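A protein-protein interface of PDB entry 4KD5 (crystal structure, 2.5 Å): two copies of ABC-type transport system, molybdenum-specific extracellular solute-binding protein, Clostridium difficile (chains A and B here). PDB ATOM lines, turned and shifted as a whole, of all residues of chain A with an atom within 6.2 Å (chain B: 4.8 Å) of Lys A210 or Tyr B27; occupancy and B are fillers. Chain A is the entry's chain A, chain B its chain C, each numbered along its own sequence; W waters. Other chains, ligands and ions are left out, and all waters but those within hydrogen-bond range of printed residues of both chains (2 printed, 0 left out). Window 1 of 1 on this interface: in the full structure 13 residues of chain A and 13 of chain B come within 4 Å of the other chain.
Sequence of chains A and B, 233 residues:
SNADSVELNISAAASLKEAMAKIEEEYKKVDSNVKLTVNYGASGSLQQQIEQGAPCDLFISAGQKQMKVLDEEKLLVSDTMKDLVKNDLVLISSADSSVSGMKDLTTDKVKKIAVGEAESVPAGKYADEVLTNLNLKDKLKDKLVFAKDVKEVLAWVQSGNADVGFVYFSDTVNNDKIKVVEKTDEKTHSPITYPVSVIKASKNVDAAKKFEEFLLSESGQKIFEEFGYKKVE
The side-chain hydroxyl of Tyr B27 lies within hydrogen-bond range of the side-chain amino group of Lys A210 (3.1 Å).
OG of Ser A217 sits close to O of Val B30, 3.4 Å away.
The side-chain amino group (NZ) of Lys A210 is in salt-bridge range of the side-chain carboxylate (OD1) of Asp B31 (3.8 Å).
The side-chain hydroxyl (OG) of Ser A217 sits at hydrogen-bond distance from the backbone NH (N) of Asp B31.
The side-chain carboxylate of Glu B26 is in salt-bridge range of the side-chain amino group of Lys B29 (3.996 Å).
CG2 of Val A30 touches CG1 of Val B30, at 3.8 Å.
Val A30 touches Phe B214.
CA of Ala A207 touches NZ of Lys B210, at 3.7 Å.
Lys A210 touches Lys B210.
O of Val B30 touches O of Glu A213, 3.999 Å away.
Glu A213 touches Asp B31 (CG to OD2, 3.9 Å).
Phe A214 touches Val B30 (CA to O, 3.6 Å).
Ser A217 touches Lys B29 (CB to O, 3.3 Å).
Of chain A, only Lys A210 comes within 4 Å of Tyr B27.
Of the printed residues of chain B, Ser A217 touches Lys B29 (3.3 Å), Val B30 (3.4 Å) and Asp B31 (3.4 Å).
Printed residues of chain B within 4 Å of Glu A213: Val B30 (3.999 Å) and Asp B31 (3.9 Å).
Of the printed residues of chain A, Asp B31 touches Lys A210, Glu A213 and Ser A217.
Printed residues of chain A within 4 Å of Lys B29: Ser A217 (3.3 Å).
The nearest residue of chain A that does not touch Tyr B27 is Val A30 (5.7 Å).
Printed residues of chain A that touch a printed residue of chain B: Val A30, Ala A207, Lys A210, Glu A213, Phe A214 and Ser A217.
Hydrophobic or aromatic side chains of chain A that line the printed part of chain B: Val A30, Ala A207 and Phe A214.
Of the 15 printed residues of chain B, 6 touch a printed residue of chain A.
Hydrophobic or aromatic side chains of chain B that line the printed part of chain A: Tyr B27, Val B30 and Phe B214.
Among the printed residues, Asp or Glu carboxylates within 4 Å of a Lys or Arg side-chain nitrogen of the other chain: Lys A210 with Asp B31 (3.8 Å).
Val B30 touches its own counterpart, Val A30.
Ala A207 touches Lys B210, but with the chains exchanged Lys A210 does not touch Ala B207 (7.1 Å).
Lys A210 touches Tyr B27, but with the chains exchanged Tyr A27 does not touch Lys B210 (5.4 Å).
Lys A210 touches Asp B31, but with the chains exchanged Asp A31 does not touch Lys B210 (4.2 Å).
Of the 12 pairs that touch across the chains among the printed residues, 4 have their exchanged pair printed and touching as well.
Water W1 bridges the backbone carbonyl oxygen of Val B30 (2.4 Å) and the side-chain amino group of Lys A210 (2.9 Å).
Water W2 lies within hydrogen-bond range of O of Ala A207, OH of Tyr A27 and NZ of Lys B210.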
ATOM      1  N   TYR A  27     -18.002  23.719  -0.612  1.00  0.00           N
ATOM      2  CA  TYR A  27     -18.126  22.322  -0.202  1.00  0.00           C
ATOM      3  C   TYR A  27     -17.269  22.035   1.033  1.00  0.00           C
ATOM      4  O   TYR A  27     -17.481  21.038   1.720  1.00  0.00           O
ATOM      5  CB  TYR A  27     -17.766  21.380  -1.356  1.00  0.00           C
ATOM      6  CG  TYR A  27     -18.164  19.943  -1.126  1.00  0.00           C
ATOM      7  CD1 TYR A  27     -19.498  19.567  -1.122  1.00  0.00           C
ATOM      8  CD2 TYR A  27     -17.208  18.961  -0.927  1.00  0.00           C
ATOM      9  CE1 TYR A  27     -19.870  18.257  -0.915  1.00  0.00           C
ATOM     10  CE2 TYR A  27     -17.570  17.647  -0.721  1.00  0.00           C
ATOM     11  CZ  TYR A  27     -18.904  17.303  -0.717  1.00  0.00           C
ATOM     12  OH  TYR A  27     -19.270  15.997  -0.514  1.00  0.00           O
ATOM     13  N   VAL A  30     -19.656  22.452   3.954  1.00  0.00           N
ATOM     14  CA  VAL A  30     -20.740  21.470   3.987  1.00  0.00           C
ATOM     15  C   VAL A  30     -20.188  20.076   4.314  1.00  0.00           C
ATOM     16  O   VAL A  30     -20.898  19.207   4.823  1.00  0.00           O
ATOM     17  CB  VAL A  30     -21.522  21.509   2.641  1.00  0.00           C
ATOM     18  CG1 VAL A  30     -22.345  20.259   2.416  1.00  0.00           C
ATOM     19  CG2 VAL A  30     -22.423  22.731   2.598  1.00  0.00           C
ATOM     20  N   ASP A  31     -18.901  19.891   4.040  1.00  0.00           N
ATOM     21  CA  ASP A  31     -18.188  18.657   4.376  1.00  0.00           C
ATOM     22  C   ASP A  31     -16.724  18.981   4.664  1.00  0.00           C
ATOM     23  O   ASP A  31     -15.952  19.264   3.748  1.00  0.00           O
ATOM     24  CB  ASP A  31     -18.278  17.645   3.225  1.00  0.00           C
ATOM     25  CG  ASP A  31     -18.039  16.211   3.678  1.00  0.00           C
ATOM     26  OD1 ASP A  31     -17.379  16.003   4.715  1.00  0.00           O
ATOM     27  OD2 ASP A  31     -18.517  15.285   2.993  1.00  0.00           O
ATOM     28  N   VAL A  34     -13.767  16.084   3.490  1.00  0.00           N
ATOM     29  CA  VAL A  34     -13.348  15.832   2.112  1.00  0.00           C
ATOM     30  C   VAL A  34     -12.328  16.865   1.647  1.00  0.00           C
ATOM     31  O   VAL A  34     -12.554  18.071   1.771  1.00  0.00           O
ATOM     32  CB  VAL A  34     -14.549  15.808   1.142  1.00  0.00           C
ATOM     33  CG1 VAL A  34     -14.080  15.881  -0.305  1.00  0.00           C
ATOM     34  CG2 VAL A  34     -15.371  14.556   1.361  1.00  0.00           C
ATOM     35  N   VAL A 205     -15.784   5.956  -4.334  1.00  0.00           N
ATOM     36  CA  VAL A 205     -17.026   6.104  -5.094  1.00  0.00           C
ATOM     37  C   VAL A 205     -18.112   6.859  -4.328  1.00  0.00           C
ATOM     38  O   VAL A 205     -18.649   7.853  -4.822  1.00  0.00           O
ATOM     39  CB  VAL A 205     -17.569   4.737  -5.568  1.00  0.00           C
ATOM     40  CG1 VAL A 205     -18.977   4.876  -6.127  1.00  0.00           C
ATOM     41  CG2 VAL A 205     -16.649   4.128  -6.613  1.00  0.00           C
ATOM     42  N   ASP A 206     -18.422   6.388  -3.123  1.00  0.00           N
ATOM     43  CA  ASP A 206     -19.451   7.013  -2.294  1.00  0.00           C
ATOM     44  C   ASP A 206     -19.162   8.482  -1.999  1.00  0.00           C
ATOM     45  O   ASP A 206     -20.038   9.330  -2.147  1.00  0.00           O
ATOM     46  CB  ASP A 206     -19.649   6.229  -0.994  1.00  0.00           C
ATOM     47  CG  ASP A 206     -20.769   5.213  -1.091  1.00  0.00           C
ATOM     48  OD1 ASP A 206     -21.787   5.513  -1.745  1.00  0.00           O
ATOM     49  OD2 ASP A 206     -20.635   4.117  -0.509  1.00  0.00           O
ATOM     50  N   ALA A 207     -17.929   8.782  -1.602  1.00  0.00           N
ATOM     51  CA  ALA A 207     -17.522  10.167  -1.376  1.00  0.00           C
ATOM     52  C   ALA A 207     -17.647  10.992  -2.655  1.00  0.00           C
ATOM     53  O   ALA A 207     -18.040  12.158  -2.616  1.00  0.00           O
ATOM     54  CB  ALA A 207     -16.108  10.231  -0.845  1.00  0.00           C
ATOM     55  N   ALA A 208     -17.312  10.381  -3.789  1.00  0.00           N
ATOM     56  CA  ALA A 208     -17.421  11.051  -5.083  1.00  0.00           C
ATOM     57  C   ALA A 208     -18.881  11.258  -5.494  1.00  0.00           C
ATOM     58  O   ALA A 208     -19.242  12.323  -6.001  1.00  0.00           O
ATOM     59  CB  ALA A 208     -16.675  10.270  -6.146  1.00  0.00           C
ATOM     60  N   LYS A 209     -19.704  10.230  -5.294  1.00  0.00           N
ATOM     61  CA  LYS A 209     -21.134  10.308  -5.588  1.00  0.00           C
ATOM     62  C   LYS A 209     -21.778  11.418  -4.773  1.00  0.00           C
ATOM     63  O   LYS A 209     -22.603  12.182  -5.273  1.00  0.00           O
ATOM     64  CB  LYS A 209     -21.827   8.980  -5.269  1.00  0.00           C
ATOM     65  CG  LYS A 209     -21.460   7.829  -6.196  1.00  0.00           C
ATOM     66  CD  LYS A 209     -22.699   7.034  -6.604  1.00  0.00           C
ATOM     67  CE  LYS A 209     -22.705   5.637  -6.009  1.00  0.00           C
ATOM     68  NZ  LYS A 209     -23.553   4.703  -6.811  1.00  0.00           N
ATOM     69  N   LYS A 210     -21.390  11.485  -3.504  1.00  0.00           N
ATOM     70  CA  LYS A 210     -21.847  12.526  -2.590  1.00  0.00           C
ATOM     71  C   LYS A 210     -21.482  13.923  -3.092  1.00  0.00           C
ATOM     72  O   LYS A 210     -22.308  14.832  -3.067  1.00  0.00           O
ATOM     73  CB  LYS A 210     -21.260  12.281  -1.195  1.00  0.00           C
ATOM     74  CG  LYS A 210     -21.165  13.509  -0.311  1.00  0.00           C
ATOM     75  CD  LYS A 210     -22.520  14.010   0.165  1.00  0.00           C
ATOM     76  CE  LYS A 210     -22.327  15.128   1.172  1.00  0.00           C
ATOM     77  NZ  LYS A 210     -23.623  15.649   1.666  1.00  0.00           N
ATOM     78  N   PHE A 211     -20.249  14.090  -3.557  1.00  0.00           N
ATOM     79  CA  PHE A 211     -19.809  15.383  -4.069  1.00  0.00           C
ATOM     80  C   PHE A 211     -20.521  15.762  -5.365  1.00  0.00           C
ATOM     81  O   PHE A 211     -20.848  16.931  -5.588  1.00  0.00           O
ATOM     82  CB  PHE A 211     -18.290  15.413  -4.263  1.00  0.00           C
ATOM     83  CG  PHE A 211     -17.791  16.686  -4.875  1.00  0.00           C
ATOM     84  CD1 PHE A 211     -18.022  17.905  -4.254  1.00  0.00           C
ATOM     85  CD2 PHE A 211     -17.099  16.669  -6.074  1.00  0.00           C
ATOM     86  CE1 PHE A 211     -17.567  19.088  -4.821  1.00  0.00           C
ATOM     87  CE2 PHE A 211     -16.640  17.846  -6.647  1.00  0.00           C
ATOM     88  CZ  PHE A 211     -16.876  19.055  -6.019  1.00  0.00           C
ATOM     89  N   GLU A 212     -20.759  14.772  -6.221  1.00  0.00           N
ATOM     90  CA  GLU A 212     -21.489  15.000  -7.466  1.00  0.00           C
ATOM     91  C   GLU A 212     -22.899  15.496  -7.154  1.00  0.00           C
ATOM     92  O   GLU A 212     -23.407  16.413  -7.804  1.00  0.00           O
ATOM     93  CB  GLU A 212     -21.549  13.722  -8.309  1.00  0.00           C
ATOM     94  CG  GLU A 212     -22.311  13.890  -9.612  1.00  0.00           C
ATOM     95  CD  GLU A 212     -22.494  12.590 -10.375  1.00  0.00           C
ATOM     96  OE1 GLU A 212     -23.541  12.442 -11.035  1.00  0.00           O
ATOM     97  OE2 GLU A 212     -21.592  11.730 -10.330  1.00  0.00           O
ATOM     98  N   GLU A 213     -23.516  14.895  -6.142  1.00  0.00           N
ATOM     99  CA  GLU A 213     -24.837  15.317  -5.691  1.00  0.00           C
ATOM    100  C   GLU A 213     -24.863  16.774  -5.239  1.00  0.00           C
ATOM    101  O   GLU A 213     -25.876  17.448  -5.387  1.00  0.00           O
ATOM    102  CB  GLU A 213     -25.363  14.395  -4.585  1.00  0.00           C
ATOM    103  CG  GLU A 213     -26.293  13.299  -5.085  1.00  0.00           C
ATOM    104  CD  GLU A 213     -27.456  13.842  -5.902  1.00  0.00           C
ATOM    105  OE1 GLU A 213     -27.948  14.951  -5.593  1.00  0.00           O
ATOM    106  OE2 GLU A 213     -27.874  13.160  -6.862  1.00  0.00           O
ATOM    107  N   PHE A 214     -23.746  17.256  -4.703  1.00  0.00           N
ATOM    108  CA  PHE A 214     -23.621  18.664  -4.333  1.00  0.00           C
ATOM    109  C   PHE A 214     -23.654  19.554  -5.573  1.00  0.00           C
ATOM    110  O   PHE A 214     -24.315  20.591  -5.585  1.00  0.00           O
ATOM    111  CB  PHE A 214     -22.331  18.910  -3.543  1.00  0.00           C
ATOM    112  CG  PHE A 214     -22.065  20.360  -3.256  1.00  0.00           C
ATOM    113  CD1 PHE A 214     -22.841  21.056  -2.340  1.00  0.00           C
ATOM    114  CD2 PHE A 214     -21.033  21.027  -3.896  1.00  0.00           C
ATOM    115  CE1 PHE A 214     -22.595  22.394  -2.075  1.00  0.00           C
ATOM    116  CE2 PHE A 214     -20.784  22.366  -3.633  1.00  0.00           C
ATOM    117  CZ  PHE A 214     -21.564  23.047  -2.723  1.00  0.00           C
ATOM    118  N   LEU A 215     -22.930  19.138  -6.607  1.00  0.00           N
ATOM    119  CA  LEU A 215     -22.922  19.838  -7.884  1.00  0.00           C
ATOM    120  C   LEU A 215     -24.323  19.840  -8.488  1.00  0.00           C
ATOM    121  O   LEU A 215     -24.782  20.849  -9.020  1.00  0.00           O
ATOM    122  CB  LEU A 215     -21.940  19.165  -8.849  1.00  0.00           C
ATOM    123  CG  LEU A 215     -20.495  18.957  -8.397  1.00  0.00           C
ATOM    124  CD1 LEU A 215     -19.752  18.054  -9.371  1.00  0.00           C
ATOM    125  CD2 LEU A 215     -19.776  20.285  -8.278  1.00  0.00           C
ATOM    126  N   SER A 217     -27.050  19.720  -6.928  1.00  0.00           N
ATOM    127  CA  SER A 217     -28.023  20.282  -5.993  1.00  0.00           C
ATOM    128  C   SER A 217     -28.169  21.793  -6.117  1.00  0.00           C
ATOM    129  O   SER A 217     -27.325  22.454  -6.724  1.00  0.00           O
ATOM    130  CB  SER A 217     -27.656  19.902  -4.564  1.00  0.00           C
ATOM    131  OG  SER A 217     -27.640  18.497  -4.433  1.00  0.00           O
ATOM    132  N   ILE B  23     -31.883  22.279   9.791  1.00  0.00           N
ATOM    133  CA  ILE B  23     -30.953  21.274   9.274  1.00  0.00           C
ATOM    134  C   ILE B  23     -31.536  20.548   8.049  1.00  0.00           C
ATOM    135  O   ILE B  23     -30.826  20.276   7.075  1.00  0.00           O
ATOM    136  CB  ILE B  23     -30.568  20.242  10.366  1.00  0.00           C
ATOM    137  CG1 ILE B  23     -29.669  20.877  11.434  1.00  0.00           C
ATOM    138  CG2 ILE B  23     -29.889  19.029   9.752  1.00  0.00           C
ATOM    139  CD1 ILE B  23     -28.300  21.291  10.930  1.00  0.00           C
ATOM    140  N   GLU B  24     -32.831  20.248   8.097  1.00  0.00           N
ATOM    141  CA  GLU B  24     -33.504  19.552   7.002  1.00  0.00           C
ATOM    142  C   GLU B  24     -33.566  20.382   5.721  1.00  0.00           C
ATOM    143  O   GLU B  24     -33.185  19.909   4.653  1.00  0.00           O
ATOM    144  CB  GLU B  24     -34.915  19.121   7.426  1.00  0.00           C
ATOM    145  CG  GLU B  24     -35.005  17.728   8.022  1.00  0.00           C
ATOM    146  CD  GLU B  24     -36.338  17.461   8.701  1.00  0.00           C
ATOM    147  OE1 GLU B  24     -37.082  16.574   8.231  1.00  0.00           O
ATOM    148  OE2 GLU B  24     -36.636  18.133   9.711  1.00  0.00           O
ATOM    149  N   GLU B  25     -34.044  21.619   5.834  1.00  0.00           N
ATOM    150  CA  GLU B  25     -34.170  22.501   4.673  1.00  0.00           C
ATOM    151  C   GLU B  25     -32.812  22.871   4.081  1.00  0.00           C
ATOM    152  O   GLU B  25     -32.701  23.137   2.885  1.00  0.00           O
ATOM    153  CB  GLU B  25     -34.972  23.764   5.024  1.00  0.00           C
ATOM    154  CG  GLU B  25     -34.129  24.994   5.377  1.00  0.00           C
ATOM    155  CD  GLU B  25     -34.214  26.080   4.318  1.00  0.00           C
ATOM    156  OE1 GLU B  25     -33.871  27.245   4.620  1.00  0.00           O
ATOM    157  OE2 GLU B  25     -34.617  25.768   3.178  1.00  0.00           O
ATOM    158  N   GLU B  26     -31.779  22.870   4.916  1.00  0.00           N
ATOM    159  CA  GLU B  26     -30.447  23.267   4.478  1.00  0.00           C
ATOM    160  C   GLU B  26     -29.681  22.110   3.849  1.00  0.00           C
ATOM    161  O   GLU B  26     -28.863  22.315   2.957  1.00  0.00           O
ATOM    162  CB  GLU B  26     -29.659  23.849   5.655  1.00  0.00           C
ATOM    163  CG  GLU B  26     -28.686  24.955   5.290  1.00  0.00           C
ATOM    164  CD  GLU B  26     -29.370  26.289   5.057  1.00  0.00           C
ATOM    165  OE1 GLU B  26     -28.658  27.291   4.837  1.00  0.00           O
ATOM    166  OE2 GLU B  26     -30.617  26.340   5.093  1.00  0.00           O
ATOM    167  N   TYR B  27     -29.945  20.893   4.317  1.00  0.00           N
ATOM    168  CA  TYR B  27     -29.309  19.712   3.745  1.00  0.00           C
ATOM    169  C   TYR B  27     -29.933  19.394   2.400  1.00  0.00           C
ATOM    170  O   TYR B  27     -29.273  18.870   1.504  1.00  0.00           O
ATOM    171  CB  TYR B  27     -29.435  18.506   4.673  1.00  0.00           C
ATOM    172  CG  TYR B  27     -28.531  17.365   4.278  1.00  0.00           C
ATOM    173  CD1 TYR B  27     -27.156  17.495   4.368  1.00  0.00           C
ATOM    174  CD2 TYR B  27     -29.047  16.163   3.817  1.00  0.00           C
ATOM    175  CE1 TYR B  27     -26.317  16.468   4.011  1.00  0.00           C
ATOM    176  CE2 TYR B  27     -28.212  15.121   3.457  1.00  0.00           C
ATOM    177  CZ  TYR B  27     -26.847  15.286   3.559  1.00  0.00           C
ATOM    178  OH  TYR B  27     -25.994  14.271   3.214  1.00  0.00           O
ATOM    179  N   LYS B  28     -31.217  19.705   2.271  1.00  0.00           N
ATOM    180  CA  LYS B  28     -31.941  19.472   1.033  1.00  0.00           C
ATOM    181  C   LYS B  28     -31.325  20.291  -0.098  1.00  0.00           C
ATOM    182  O   LYS B  28     -31.342  19.874  -1.257  1.00  0.00           O
ATOM    183  CB  LYS B  28     -33.422  19.821   1.213  1.00  0.00           C
ATOM    184  CG  LYS B  28     -34.302  19.433   0.036  1.00  0.00           C
ATOM    185  CD  LYS B  28     -34.213  17.939  -0.250  1.00  0.00           C
ATOM    186  CE  LYS B  28     -34.927  17.583  -1.546  1.00  0.00           C
ATOM    187  NZ  LYS B  28     -34.844  16.123  -1.833  1.00  0.00           N
ATOM    188  N   LYS B  29     -30.761  21.444   0.253  1.00  0.00           N
ATOM    189  CA  LYS B  29     -30.153  22.343  -0.726  1.00  0.00           C
ATOM    190  C   LYS B  29     -28.791  21.859  -1.221  1.00  0.00           C
ATOM    191  O   LYS B  29     -28.347  22.246  -2.298  1.00  0.00           O
ATOM    192  CB  LYS B  29     -30.041  23.756  -0.146  1.00  0.00           C
ATOM    193  CG  LYS B  29     -31.381  24.443   0.036  1.00  0.00           C
ATOM    194  CD  LYS B  29     -31.332  25.566   1.072  1.00  0.00           C
ATOM    195  CE  LYS B  29     -30.474  26.736   0.624  1.00  0.00           C
ATOM    196  NZ  LYS B  29     -30.740  27.958   1.441  1.00  0.00           N
ATOM    197  N   VAL B  30     -28.143  21.006  -0.432  1.00  0.00           N
ATOM    198  CA  VAL B  30     -26.828  20.468  -0.788  1.00  0.00           C
ATOM    199  C   VAL B  30     -26.866  18.978  -1.148  1.00  0.00           C
ATOM    200  O   VAL B  30     -25.845  18.393  -1.501  1.00  0.00           O
ATOM    201  CB  VAL B  30     -25.786  20.713   0.329  1.00  0.00           C
ATOM    202  CG1 VAL B  30     -25.509  22.198   0.483  1.00  0.00           C
ATOM    203  CG2 VAL B  30     -26.277  20.134   1.644  1.00  0.00           C
ATOM    204  N   ASP B  31     -28.049  18.375  -1.053  1.00  0.00           N
ATOM    205  CA  ASP B  31     -28.243  16.968  -1.410  1.00  0.00           C
ATOM    206  C   ASP B  31     -29.726  16.667  -1.631  1.00  0.00           C
ATOM    207  O   ASP B  31     -30.442  16.344  -0.684  1.00  0.00           O
ATOM    208  CB  ASP B  31     -27.688  16.055  -0.309  1.00  0.00           C
ATOM    209  CG  ASP B  31     -27.430  14.640  -0.793  1.00  0.00           C
ATOM    210  OD1 ASP B  31     -26.505  13.993  -0.262  1.00  0.00           O
ATOM    211  OD2 ASP B  31     -28.139  14.174  -1.710  1.00  0.00           O
ATOM    212  N   VAL B  34     -31.625  12.913  -0.590  1.00  0.00           N
ATOM    213  CA  VAL B  34     -31.914  12.389   0.741  1.00  0.00           C
ATOM    214  C   VAL B  34     -33.195  12.975   1.318  1.00  0.00           C
ATOM    215  O   VAL B  34     -33.375  14.195   1.338  1.00  0.00           O
ATOM    216  CB  VAL B  34     -30.744  12.632   1.714  1.00  0.00           C
ATOM    217  CG1 VAL B  34     -31.080  12.100   3.101  1.00  0.00           C
ATOM    218  CG2 VAL B  34     -29.492  11.963   1.195  1.00  0.00           C
ATOM    219  N   LEU B  36     -35.184  13.121   4.857  1.00  0.00           N
ATOM    220  CA  LEU B  36     -34.961  12.888   6.281  1.00  0.00           C
ATOM    221  C   LEU B  36     -36.283  12.734   7.033  1.00  0.00           C
ATOM    222  O   LEU B  36     -37.202  13.539   6.860  1.00  0.00           O
ATOM    223  CB  LEU B  36     -34.143  14.032   6.890  1.00  0.00           C
ATOM    224  CG  LEU B  36     -32.746  14.300   6.332  1.00  0.00           C
ATOM    225  CD1 LEU B  36     -32.147  15.554   6.951  1.00  0.00           C
ATOM    226  CD2 LEU B  36     -31.830  13.119   6.579  1.00  0.00           C
ATOM    227  N   ALA B 207     -24.812   6.868   3.644  1.00  0.00           N
ATOM    228  CA  ALA B 207     -25.695   8.030   3.571  1.00  0.00           C
ATOM    229  C   ALA B 207     -25.831   8.697   4.943  1.00  0.00           C
ATOM    230  O   ALA B 207     -25.971   9.917   5.043  1.00  0.00           O
ATOM    231  CB  ALA B 207     -27.051   7.631   3.039  1.00  0.00           C
ATOM    232  N   LYS B 210     -22.524  10.552   5.802  1.00  0.00           N
ATOM    233  CA  LYS B 210     -22.458  11.790   5.033  1.00  0.00           C
ATOM    234  C   LYS B 210     -23.350  12.875   5.629  1.00  0.00           C
ATOM    235  O   LYS B 210     -22.989  14.048   5.630  1.00  0.00           O
ATOM    236  CB  LYS B 210     -22.829  11.545   3.567  1.00  0.00           C
ATOM    237  CG  LYS B 210     -21.641  11.378   2.627  1.00  0.00           C
ATOM    238  CD  LYS B 210     -20.751  10.207   3.016  1.00  0.00           C
ATOM    239  CE  LYS B 210     -19.585  10.048   2.046  1.00  0.00           C
ATOM    240  NZ  LYS B 210     -18.717  11.263   1.986  1.00  0.00           N
ATOM    241  N   PHE B 211     -24.517  12.487   6.132  1.00  0.00           N
ATOM    242  CA  PHE B 211     -25.389  13.450   6.791  1.00  0.00           C
ATOM    243  C   PHE B 211     -24.822  13.871   8.138  1.00  0.00           C
ATOM    244  O   PHE B 211     -25.014  15.004   8.569  1.00  0.00           O
ATOM    245  CB  PHE B 211     -26.811  12.913   6.969  1.00  0.00           C
ATOM    246  CG  PHE B 211     -27.695  13.824   7.776  1.00  0.00           C
ATOM    247  CD1 PHE B 211     -28.011  15.095   7.313  1.00  0.00           C
ATOM    248  CD2 PHE B 211     -28.203  13.417   9.000  1.00  0.00           C
ATOM    249  CE1 PHE B 211     -28.822  15.940   8.058  1.00  0.00           C
ATOM    250  CE2 PHE B 211     -29.016  14.257   9.747  1.00  0.00           C
ATOM    251  CZ  PHE B 211     -29.324  15.518   9.275  1.00  0.00           C
ATOM    252  N   PHE B 214     -22.324  16.621   7.688  1.00  0.00           N
ATOM    253  CA  PHE B 214     -22.933  17.924   7.446  1.00  0.00           C
ATOM    254  C   PHE B 214     -23.184  18.610   8.782  1.00  0.00           C
ATOM    255  O   PHE B 214     -22.999  19.816   8.922  1.00  0.00           O
ATOM    256  CB  PHE B 214     -24.246  17.799   6.671  1.00  0.00           C
ATOM    257  CG  PHE B 214     -25.018  19.085   6.585  1.00  0.00           C
ATOM    258  CD1 PHE B 214     -24.561  20.131   5.797  1.00  0.00           C
ATOM    259  CD2 PHE B 214     -26.201  19.249   7.291  1.00  0.00           C
ATOM    260  CE1 PHE B 214     -25.268  21.324   5.716  1.00  0.00           C
ATOM    261  CE2 PHE B 214     -26.916  20.437   7.215  1.00  0.00           C
ATOM    262  CZ  PHE B 214     -26.447  21.476   6.424  1.00  0.00           C
HETATM  263  O   HOH W   1     -24.038  16.846  -0.984  1.00  0.00           O
HETATM  264  O   HOH W   2     -17.962  13.635  -0.421  1.00  0.00           O
